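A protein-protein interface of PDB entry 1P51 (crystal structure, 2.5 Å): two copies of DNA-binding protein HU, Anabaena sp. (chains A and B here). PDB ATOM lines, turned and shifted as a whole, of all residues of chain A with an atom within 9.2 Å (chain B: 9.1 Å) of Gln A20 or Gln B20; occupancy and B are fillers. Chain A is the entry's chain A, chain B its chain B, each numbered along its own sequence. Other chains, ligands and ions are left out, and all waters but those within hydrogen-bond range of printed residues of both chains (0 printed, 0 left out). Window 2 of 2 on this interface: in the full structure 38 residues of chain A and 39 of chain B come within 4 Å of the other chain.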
ATOM      1  N   VAL A   7       8.025   2.495  23.813  1.00  0.00           N
ATOM      2  CA  VAL A   7       9.210   1.674  24.066  1.00  0.00           C
ATOM      3  C   VAL A   7       8.971   0.692  25.219  1.00  0.00           C
ATOM      4  O   VAL A   7       9.223  -0.506  25.076  1.00  0.00           O
ATOM      5  CB  VAL A   7      10.466   2.551  24.332  1.00  0.00           C
ATOM      6  CG1 VAL A   7      11.604   1.728  24.916  1.00  0.00           C
ATOM      7  CG2 VAL A   7      10.919   3.250  23.054  1.00  0.00           C
ATOM      8  N   VAL A  10       6.651  -2.024  24.120  1.00  0.00           N
ATOM      9  CA  VAL A  10       7.363  -2.840  23.138  1.00  0.00           C
ATOM     10  C   VAL A  10       8.372  -3.767  23.823  1.00  0.00           C
ATOM     11  O   VAL A  10       8.402  -4.969  23.549  1.00  0.00           O
ATOM     12  CB  VAL A  10       8.069  -1.955  22.072  1.00  0.00           C
ATOM     13  CG1 VAL A  10       9.061  -2.762  21.246  1.00  0.00           C
ATOM     14  CG2 VAL A  10       7.046  -1.295  21.162  1.00  0.00           C
ATOM     15  N   ALA A  11       9.182  -3.198  24.718  1.00  0.00           N
ATOM     16  CA  ALA A  11      10.171  -3.950  25.489  1.00  0.00           C
ATOM     17  C   ALA A  11       9.513  -5.050  26.319  1.00  0.00           C
ATOM     18  O   ALA A  11      10.068  -6.139  26.471  1.00  0.00           O
ATOM     19  CB  ALA A  11      10.972  -3.014  26.382  1.00  0.00           C
ATOM     20  N   ALA A  14       7.953  -7.736  23.387  1.00  0.00           N
ATOM     21  CA  ALA A  14       8.999  -8.452  22.655  1.00  0.00           C
ATOM     22  C   ALA A  14       9.979  -9.190  23.569  1.00  0.00           C
ATOM     23  O   ALA A  14      10.827  -9.951  23.090  1.00  0.00           O
ATOM     24  CB  ALA A  14       9.745  -7.495  21.734  1.00  0.00           C
ATOM     25  N   SER A  15       9.847  -8.968  24.878  1.00  0.00           N
ATOM     26  CA  SER A  15      10.737  -9.547  25.891  1.00  0.00           C
ATOM     27  C   SER A  15      12.199  -9.159  25.650  1.00  0.00           C
ATOM     28  O   SER A  15      13.084 -10.017  25.564  1.00  0.00           O
ATOM     29  CB  SER A  15      10.562 -11.071  25.988  1.00  0.00           C
ATOM     30  OG  SER A  15       9.202 -11.419  26.182  1.00  0.00           O
ATOM     31  N   VAL A  16      12.428  -7.853  25.523  1.00  0.00           N
ATOM     32  CA  VAL A  16      13.764  -7.279  25.364  1.00  0.00           C
ATOM     33  C   VAL A  16      13.929  -6.089  26.313  1.00  0.00           C
ATOM     34  O   VAL A  16      12.963  -5.656  26.945  1.00  0.00           O
ATOM     35  CB  VAL A  16      14.050  -6.835  23.897  1.00  0.00           C
ATOM     36  CG1 VAL A  16      14.208  -8.043  22.978  1.00  0.00           C
ATOM     37  CG2 VAL A  16      12.965  -5.887  23.373  1.00  0.00           C
ATOM     38  N   THR A  17      15.150  -5.569  26.416  1.00  0.00           N
ATOM     39  CA  THR A  17      15.416  -4.389  27.240  1.00  0.00           C
ATOM     40  C   THR A  17      14.922  -3.105  26.564  1.00  0.00           C
ATOM     41  O   THR A  17      14.791  -3.052  25.338  1.00  0.00           O
ATOM     42  CB  THR A  17      16.921  -4.292  27.627  1.00  0.00           C
ATOM     43  OG1 THR A  17      17.203  -2.993  28.166  1.00  0.00           O
ATOM     44  CG2 THR A  17      17.821  -4.366  26.400  1.00  0.00           C
ATOM     45  N   LYS A  18      14.648  -2.084  27.375  1.00  0.00           N
ATOM     46  CA  LYS A  18      14.115  -0.808  26.890  1.00  0.00           C
ATOM     47  C   LYS A  18      15.056  -0.110  25.909  1.00  0.00           C
ATOM     48  O   LYS A  18      14.605   0.514  24.949  1.00  0.00           O
ATOM     49  CB  LYS A  18      13.792   0.123  28.062  1.00  0.00           C
ATOM     50  CG  LYS A  18      12.491  -0.206  28.784  1.00  0.00           C
ATOM     51  CD  LYS A  18      12.414   0.523  30.118  1.00  0.00           C
ATOM     52  CE  LYS A  18      11.350  -0.079  31.016  1.00  0.00           C
ATOM     53  NZ  LYS A  18      11.166   0.706  32.266  1.00  0.00           N
ATOM     54  N   LYS A  19      16.360  -0.226  26.163  1.00  0.00           N
ATOM     55  CA  LYS A  19      17.389   0.333  25.290  1.00  0.00           C
ATOM     56  C   LYS A  19      17.369  -0.334  23.917  1.00  0.00           C
ATOM     57  O   LYS A  19      17.521   0.337  22.894  1.00  0.00           O
ATOM     58  CB  LYS A  19      18.770   0.179  25.935  1.00  0.00           C
ATOM     59  CG  LYS A  19      19.865   1.026  25.301  1.00  0.00           C
ATOM     60  CD  LYS A  19      21.227   0.679  25.876  1.00  0.00           C
ATOM     61  CE  LYS A  19      22.287   0.624  24.789  1.00  0.00           C
ATOM     62  NZ  LYS A  19      22.375  -0.730  24.171  1.00  0.00           N
ATOM     63  N   GLN A  20      17.171  -1.651  23.910  1.00  0.00           N
ATOM     64  CA  GLN A  20      17.111  -2.446  22.684  1.00  0.00           C
ATOM     65  C   GLN A  20      15.840  -2.159  21.885  1.00  0.00           C
ATOM     66  O   GLN A  20      15.879  -2.084  20.656  1.00  0.00           O
ATOM     67  CB  GLN A  20      17.198  -3.935  23.019  1.00  0.00           C
ATOM     68  CG  GLN A  20      17.526  -4.848  21.843  1.00  0.00           C
ATOM     69  CD  GLN A  20      18.090  -6.194  22.280  1.00  0.00           C
ATOM     70  OE1 GLN A  20      18.969  -6.746  21.614  1.00  0.00           O
ATOM     71  NE2 GLN A  20      17.584  -6.726  23.394  1.00  0.00           N
ATOM     72  N   ALA A  21      14.721  -2.012  22.594  1.00  0.00           N
ATOM     73  CA  ALA A  21      13.438  -1.668  21.983  1.00  0.00           C
ATOM     74  C   ALA A  21      13.486  -0.291  21.321  1.00  0.00           C
ATOM     75  O   ALA A  21      12.929  -0.101  20.237  1.00  0.00           O
ATOM     76  CB  ALA A  21      12.325  -1.722  23.022  1.00  0.00           C
ATOM     77  N   ASP A  22      14.158   0.654  21.980  1.00  0.00           N
ATOM     78  CA  ASP A  22      14.339   2.008  21.460  1.00  0.00           C
ATOM     79  C   ASP A  22      15.297   2.037  20.269  1.00  0.00           C
ATOM     80  O   ASP A  22      15.043   2.736  19.287  1.00  0.00           O
ATOM     81  CB  ASP A  22      14.834   2.950  22.566  1.00  0.00           C
ATOM     82  CG  ASP A  22      15.038   4.377  22.077  1.00  0.00           C
ATOM     83  OD1 ASP A  22      16.105   4.667  21.490  1.00  0.00           O
ATOM     84  OD2 ASP A  22      14.186   5.279  22.236  1.00  0.00           O
ATOM     85  N   ALA A  23      16.393   1.282  20.366  1.00  0.00           N
ATOM     86  CA  ALA A  23      17.404   1.226  19.307  1.00  0.00           C
ATOM     87  C   ALA A  23      16.814   0.729  17.992  1.00  0.00           C
ATOM     88  O   ALA A  23      17.098   1.282  16.926  1.00  0.00           O
ATOM     89  CB  ALA A  23      18.577   0.351  19.730  1.00  0.00           C
ATOM     90  N   VAL A  24      15.988  -0.311  18.085  1.00  0.00           N
ATOM     91  CA  VAL A  24      15.302  -0.884  16.932  1.00  0.00           C
ATOM     92  C   VAL A  24      14.247   0.085  16.393  1.00  0.00           C
ATOM     93  O   VAL A  24      14.208   0.355  15.190  1.00  0.00           O
ATOM     94  CB  VAL A  24      14.671  -2.259  17.277  1.00  0.00           C
ATOM     95  CG1 VAL A  24      13.672  -2.696  16.212  1.00  0.00           C
ATOM     96  CG2 VAL A  24      15.755  -3.317  17.453  1.00  0.00           C
ATOM     97  N   LEU A  25      13.411   0.615  17.288  1.00  0.00           N
ATOM     98  CA  LEU A  25      12.343   1.544  16.913  1.00  0.00           C
ATOM     99  C   LEU A  25      12.879   2.787  16.202  1.00  0.00           C
ATOM    100  O   LEU A  25      12.327   3.204  15.181  1.00  0.00           O
ATOM    101  CB  LEU A  25      11.500   1.935  18.138  1.00  0.00           C
ATOM    102  CG  LEU A  25      10.290   2.856  17.941  1.00  0.00           C
ATOM    103  CD1 LEU A  25       9.121   2.123  17.298  1.00  0.00           C
ATOM    104  CD2 LEU A  25       9.870   3.476  19.263  1.00  0.00           C
ATOM    105  N   THR A  26      13.953   3.364  16.741  1.00  0.00           N
ATOM    106  CA  THR A  26      14.635   4.498  16.114  1.00  0.00           C
ATOM    107  C   THR A  26      15.098   4.142  14.699  1.00  0.00           C
ATOM    108  O   THR A  26      14.785   4.854  13.742  1.00  0.00           O
ATOM    109  CB  THR A  26      15.829   4.965  16.981  1.00  0.00           C
ATOM    110  OG1 THR A  26      15.350   5.402  18.260  1.00  0.00           O
ATOM    111  CG2 THR A  26      16.463   6.221  16.406  1.00  0.00           C
ATOM    112  N   ALA A  27      15.825   3.030  14.581  1.00  0.00           N
ATOM    113  CA  ALA A  27      16.324   2.541  13.297  1.00  0.00           C
ATOM    114  C   ALA A  27      15.195   2.272  12.301  1.00  0.00           C
ATOM    115  O   ALA A  27      15.308   2.611  11.124  1.00  0.00           O
ATOM    116  CB  ALA A  27      17.167   1.287  13.498  1.00  0.00           C
ATOM    117  N   ALA A  28      14.110   1.671  12.789  1.00  0.00           N
ATOM    118  CA  ALA A  28      12.943   1.360  11.965  1.00  0.00           C
ATOM    119  C   ALA A  28      12.289   2.614  11.393  1.00  0.00           C
ATOM    120  O   ALA A  28      11.990   2.667  10.203  1.00  0.00           O
ATOM    121  CB  ALA A  28      11.933   0.539  12.759  1.00  0.00           C
ATOM    122  N   VAL B   7      13.345  -5.150   8.121  1.00  0.00           N
ATOM    123  CA  VAL B   7      13.934  -5.907   9.231  1.00  0.00           C
ATOM    124  C   VAL B   7      15.441  -6.109   9.038  1.00  0.00           C
ATOM    125  O   VAL B   7      16.224  -5.916   9.972  1.00  0.00           O
ATOM    126  CB  VAL B   7      13.218  -7.276   9.430  1.00  0.00           C
ATOM    127  CG1 VAL B   7      14.026  -8.196  10.343  1.00  0.00           C
ATOM    128  CG2 VAL B   7      11.818  -7.072  10.002  1.00  0.00           C
ATOM    129  N   VAL B  10      17.182  -2.903   9.735  1.00  0.00           N
ATOM    130  CA  VAL B  10      17.045  -2.594  11.159  1.00  0.00           C
ATOM    131  C   VAL B  10      17.993  -3.453  11.998  1.00  0.00           C
ATOM    132  O   VAL B  10      18.680  -2.940  12.885  1.00  0.00           O
ATOM    133  CB  VAL B  10      15.579  -2.756  11.644  1.00  0.00           C
ATOM    134  CG1 VAL B  10      15.496  -2.737  13.162  1.00  0.00           C
ATOM    135  CG2 VAL B  10      14.702  -1.661  11.065  1.00  0.00           C
ATOM    136  N   ALA B  11      18.029  -4.754  11.703  1.00  0.00           N
ATOM    137  CA  ALA B  11      18.948  -5.687  12.356  1.00  0.00           C
ATOM    138  C   ALA B  11      20.403  -5.295  12.110  1.00  0.00           C
ATOM    139  O   ALA B  11      21.267  -5.518  12.960  1.00  0.00           O
ATOM    140  CB  ALA B  11      18.691  -7.108  11.880  1.00  0.00           C
ATOM    141  N   ALA B  14      20.727  -1.524  14.168  1.00  0.00           N
ATOM    142  CA  ALA B  14      20.663  -1.659  15.623  1.00  0.00           C
ATOM    143  C   ALA B  14      21.651  -2.692  16.174  1.00  0.00           C
ATOM    144  O   ALA B  14      21.777  -2.848  17.393  1.00  0.00           O
ATOM    145  CB  ALA B  14      19.239  -1.988  16.063  1.00  0.00           C
ATOM    146  N   SER B  15      22.354  -3.377  15.270  1.00  0.00           N
ATOM    147  CA  SER B  15      23.311  -4.433  15.619  1.00  0.00           C
ATOM    148  C   SER B  15      22.661  -5.557  16.434  1.00  0.00           C
ATOM    149  O   SER B  15      23.165  -5.960  17.489  1.00  0.00           O
ATOM    150  CB  SER B  15      24.543  -3.855  16.333  1.00  0.00           C
ATOM    151  OG  SER B  15      25.233  -2.940  15.498  1.00  0.00           O
ATOM    152  N   VAL B  16      21.530  -6.047  15.930  1.00  0.00           N
ATOM    153  CA  VAL B  16      20.804  -7.163  16.537  1.00  0.00           C
ATOM    154  C   VAL B  16      20.493  -8.222  15.476  1.00  0.00           C
ATOM    155  O   VAL B  16      20.802  -8.031  14.298  1.00  0.00           O
ATOM    156  CB  VAL B  16      19.494  -6.697  17.240  1.00  0.00           C
ATOM    157  CG1 VAL B  16      19.809  -5.861  18.474  1.00  0.00           C
ATOM    158  CG2 VAL B  16      18.582  -5.931  16.276  1.00  0.00           C
ATOM    159  N   THR B  17      19.895  -9.336  15.893  1.00  0.00           N
ATOM    160  CA  THR B  17      19.509 -10.391  14.955  1.00  0.00           C
ATOM    161  C   THR B  17      18.185 -10.069  14.255  1.00  0.00           C
ATOM    162  O   THR B  17      17.369  -9.301  14.770  1.00  0.00           O
ATOM    163  CB  THR B  17      19.474 -11.792  15.641  1.00  0.00           C
ATOM    164  OG1 THR B  17      18.656 -12.689  14.876  1.00  0.00           O
ATOM    165  CG2 THR B  17      18.772 -11.740  16.992  1.00  0.00           C
ATOM    166  N   LYS B  18      17.994 -10.658  13.075  1.00  0.00           N
ATOM    167  CA  LYS B  18      16.799 -10.441  12.260  1.00  0.00           C
ATOM    168  C   LYS B  18      15.529 -10.944  12.948  1.00  0.00           C
ATOM    169  O   LYS B  18      14.463 -10.344  12.807  1.00  0.00           O
ATOM    170  CB  LYS B  18      16.953 -11.111  10.891  1.00  0.00           C
ATOM    171  CG  LYS B  18      17.916 -10.406   9.946  1.00  0.00           C
ATOM    172  CD  LYS B  18      18.107 -11.213   8.670  1.00  0.00           C
ATOM    173  CE  LYS B  18      19.462 -10.945   8.033  1.00  0.00           C
ATOM    174  NZ  LYS B  18      19.669 -11.773   6.810  1.00  0.00           N
ATOM    175  N   LYS B  19      15.657 -12.046  13.687  1.00  0.00           N
ATOM    176  CA  LYS B  19      14.561 -12.609  14.473  1.00  0.00           C
ATOM    177  C   LYS B  19      14.133 -11.660  15.593  1.00  0.00           C
ATOM    178  O   LYS B  19      12.949 -11.582  15.927  1.00  0.00           O
ATOM    179  CB  LYS B  19      14.970 -13.963  15.060  1.00  0.00           C
ATOM    180  CG  LYS B  19      13.803 -14.871  15.433  1.00  0.00           C
ATOM    181  CD  LYS B  19      14.244 -15.940  16.426  1.00  0.00           C
ATOM    182  CE  LYS B  19      13.301 -16.014  17.622  1.00  0.00           C
ATOM    183  NZ  LYS B  19      13.654 -15.023  18.680  1.00  0.00           N
ATOM    184  N   GLN B  20      15.105 -10.949  16.163  1.00  0.00           N
ATOM    185  CA  GLN B  20      14.856  -9.948  17.199  1.00  0.00           C
ATOM    186  C   GLN B  20      14.245  -8.685  16.597  1.00  0.00           C
ATOM    187  O   GLN B  20      13.232  -8.187  17.090  1.00  0.00           O
ATOM    188  CB  GLN B  20      16.158  -9.609  17.930  1.00  0.00           C
ATOM    189  CG  GLN B  20      15.991  -8.843  19.239  1.00  0.00           C
ATOM    190  CD  GLN B  20      17.187  -8.999  20.170  1.00  0.00           C
ATOM    191  OE1 GLN B  20      17.016  -9.123  21.383  1.00  0.00           O
ATOM    192  NE2 GLN B  20      18.393  -8.988  19.608  1.00  0.00           N
ATOM    193  N   ALA B  21      14.868  -8.181  15.530  1.00  0.00           N
ATOM    194  CA  ALA B  21      14.405  -6.976  14.836  1.00  0.00           C
ATOM    195  C   ALA B  21      12.948  -7.087  14.386  1.00  0.00           C
ATOM    196  O   ALA B  21      12.189  -6.123  14.492  1.00  0.00           O
ATOM    197  CB  ALA B  21      15.310  -6.662  13.650  1.00  0.00           C
ATOM    198  N   ASP B  22      12.572  -8.268  13.894  1.00  0.00           N
ATOM    199  CA  ASP B  22      11.195  -8.563  13.502  1.00  0.00           C
ATOM    200  C   ASP B  22      10.265  -8.591  14.713  1.00  0.00           C
ATOM    201  O   ASP B  22       9.206  -7.964  14.693  1.00  0.00           O
ATOM    202  CB  ASP B  22      11.122  -9.897  12.744  1.00  0.00           C
ATOM    203  CG  ASP B  22       9.702 -10.264  12.325  1.00  0.00           C
ATOM    204  OD1 ASP B  22       8.897 -10.655  13.201  1.00  0.00           O
ATOM    205  OD2 ASP B  22       9.302 -10.200  11.143  1.00  0.00           O
ATOM    206  N   ALA B  23      10.667  -9.321  15.755  1.00  0.00           N
ATOM    207  CA  ALA B  23       9.852  -9.495  16.960  1.00  0.00           C
ATOM    208  C   ALA B  23       9.511  -8.165  17.623  1.00  0.00           C
ATOM    209  O   ALA B  23       8.400  -7.984  18.128  1.00  0.00           O
ATOM    210  CB  ALA B  23      10.552 -10.419  17.948  1.00  0.00           C
ATOM    211  N   VAL B  24      10.473  -7.246  17.611  1.00  0.00           N
ATOM    212  CA  VAL B  24      10.297  -5.908  18.166  1.00  0.00           C
ATOM    213  C   VAL B  24       9.404  -5.057  17.256  1.00  0.00           C
ATOM    214  O   VAL B  24       8.469  -4.412  17.733  1.00  0.00           O
ATOM    215  CB  VAL B  24      11.665  -5.212  18.416  1.00  0.00           C
ATOM    216  CG1 VAL B  24      11.479  -3.749  18.795  1.00  0.00           C
ATOM    217  CG2 VAL B  24      12.443  -5.940  19.503  1.00  0.00           C
ATOM    218  N   LEU B  25       9.691  -5.071  15.954  1.00  0.00           N
ATOM    219  CA  LEU B  25       8.903  -4.330  14.967  1.00  0.00           C
ATOM    220  C   LEU B  25       7.443  -4.786  14.959  1.00  0.00           C
ATOM    221  O   LEU B  25       6.535  -3.956  14.893  1.00  0.00           O
ATOM    222  CB  LEU B  25       9.524  -4.450  13.567  1.00  0.00           C
ATOM    223  CG  LEU B  25       8.921  -3.665  12.394  1.00  0.00           C
ATOM    224  CD1 LEU B  25       9.055  -2.156  12.578  1.00  0.00           C
ATOM    225  CD2 LEU B  25       9.558  -4.103  11.080  1.00  0.00           C
ATOM    226  N   THR B  26       7.231  -6.100  15.037  1.00  0.00           N
ATOM    227  CA  THR B  26       5.894  -6.679  15.173  1.00  0.00           C
ATOM    228  C   THR B  26       5.182  -6.114  16.404  1.00  0.00           C
ATOM    229  O   THR B  26       4.047  -5.641  16.307  1.00  0.00           O
ATOM    230  CB  THR B  26       5.969  -8.224  15.252  1.00  0.00           C
ATOM    231  OG1 THR B  26       6.660  -8.731  14.100  1.00  0.00           O
ATOM    232  CG2 THR B  26       4.582  -8.846  15.129  1.00  0.00           C
ATOM    233  N   ALA B  27       5.862  -6.154  17.550  1.00  0.00           N
ATOM    234  CA  ALA B  27       5.336  -5.603  18.798  1.00  0.00           C
ATOM    235  C   ALA B  27       5.026  -4.108  18.683  1.00  0.00           C
ATOM    236  O   ALA B  27       3.974  -3.657  19.133  1.00  0.00           O
ATOM    237  CB  ALA B  27       6.303  -5.861  19.948  1.00  0.00           C
ATOM    238  N   ALA B  28       5.943  -3.360  18.072  1.00  0.00           N
ATOM    239  CA  ALA B  28       5.792  -1.917  17.880  1.00  0.00           C
ATOM    240  C   ALA B  28       4.563  -1.558  17.042  1.00  0.00           C
ATOM    241  O   ALA B  28       3.809  -0.650  17.395  1.00  0.00           O
ATOM    242  CB  ALA B  28       7.060  -1.326  17.259  1.00  0.00           C
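Ala A14 touches Ala B23, but with the chains exchanged Ala A23 does not touch Ala B14 (4.003 Å).
Ala A14 touches Val B24, and with the chains exchanged Val A24 touches Ala B14.
Val A16 touches Val B24, but with the chains exchanged Val A24 does not touch Val B16 (4.03 Å).
Ala A28 touches Leu B25, but with the chains exchanged Leu A25 does not touch Ala B28 (4.02 Å).
18 positions are printed for both chains.
Of the 13 pairs that touch across the chains among the printed residues, 10 have their exchanged pair printed and touching as well.
Of chain B, only Val B16 and Gln B20 come within 4 Å of Gln A20.
Of the printed residues of chain A, Gln B20 touches Val A16 (3.4 Å) and Gln A20 (3.1 Å).
No residue of chain B comes within 4 Å of Thr A17.
Thr B17 touches none of the printed residues of chain A.
No residue of chain A comes within 4 Å of Ala B21.
Of the printed residues of chain B, Ala A14 touches Ala B23 and Val B24.
Of the printed residues of chain B, Ala A28 touches Val B10 (3.6 Å) and Leu B25 (3.9 Å).
Of the printed residues of chain A, Val B16 touches Gln A20.
Printed residues of chain A within 4 Å of Ala B28: Val A10 (3.6 Å).
Lys B19 touches none of the printed residues of chain A.
Val A7 touches none of the printed residues of chain B.
The nearest residue of chain B that does not touch Gln A20 is Val B24 (5.1 Å).
The nearest residue of chain A that does not touch Gln B20 is Val A24 (5.5 Å).
The nearest printed residue of chain B that does not touch Val A10 is Ala B27 (4.3 Å).
O of Ala A11 lies within hydrogen-bond range of N of Val A16 (3.1 Å).
The backbone carbonyl oxygen of Ala B11 lies within hydrogen-bond range of the backbone NH of Val B16 (3.0 Å).
Among the printed residues, merely in contact across the chains: Val A10 with Val B24 (3.6 Å), Val A10 with Ala B28 (3.6 Å), Ala A14 with Ala B23 (3.9 Å), Ala A14 with Val B24 (3.8 Å), Val A16 with Gln B20 (3.4 Å), Val A16 with Val B24 (3.9 Å), Gln A20 with Val B16 (3.4 Å), Val A24 with Val B10 (3.6 Å), Val A24 with Ala B14 (3.98 Å), Val A24 with Val B24 (3.5 Å), Ala A28 with Val B10 (3.6 Å) and Ala A28 with Leu B25 (3.9 Å).
The side-chain amide oxygen (OE1) of Gln A20 is in hydrogen-bond range of the side-chain amide nitrogen (NE2) of Gln B20, at 3.1 Å.
Of the 18 printed residues of chain B, 8 touch a printed residue of chain A.
Hydrophobic or aromatic side chains of chain B that line the printed part of chain A: Val B10, Ala B14, Val B16, Val B24, Leu B25 and Ala B28.
Along chain B the printed residues that touch a printed residue of chain A span positions 10 to 28.
Hydrophobic or aromatic side chains of chain A that line the printed part of chain B: Val A10, Ala A14, Val A16, Val A24 and Ala A28.
Among the printed residues, 13 pairs touch across the chains.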
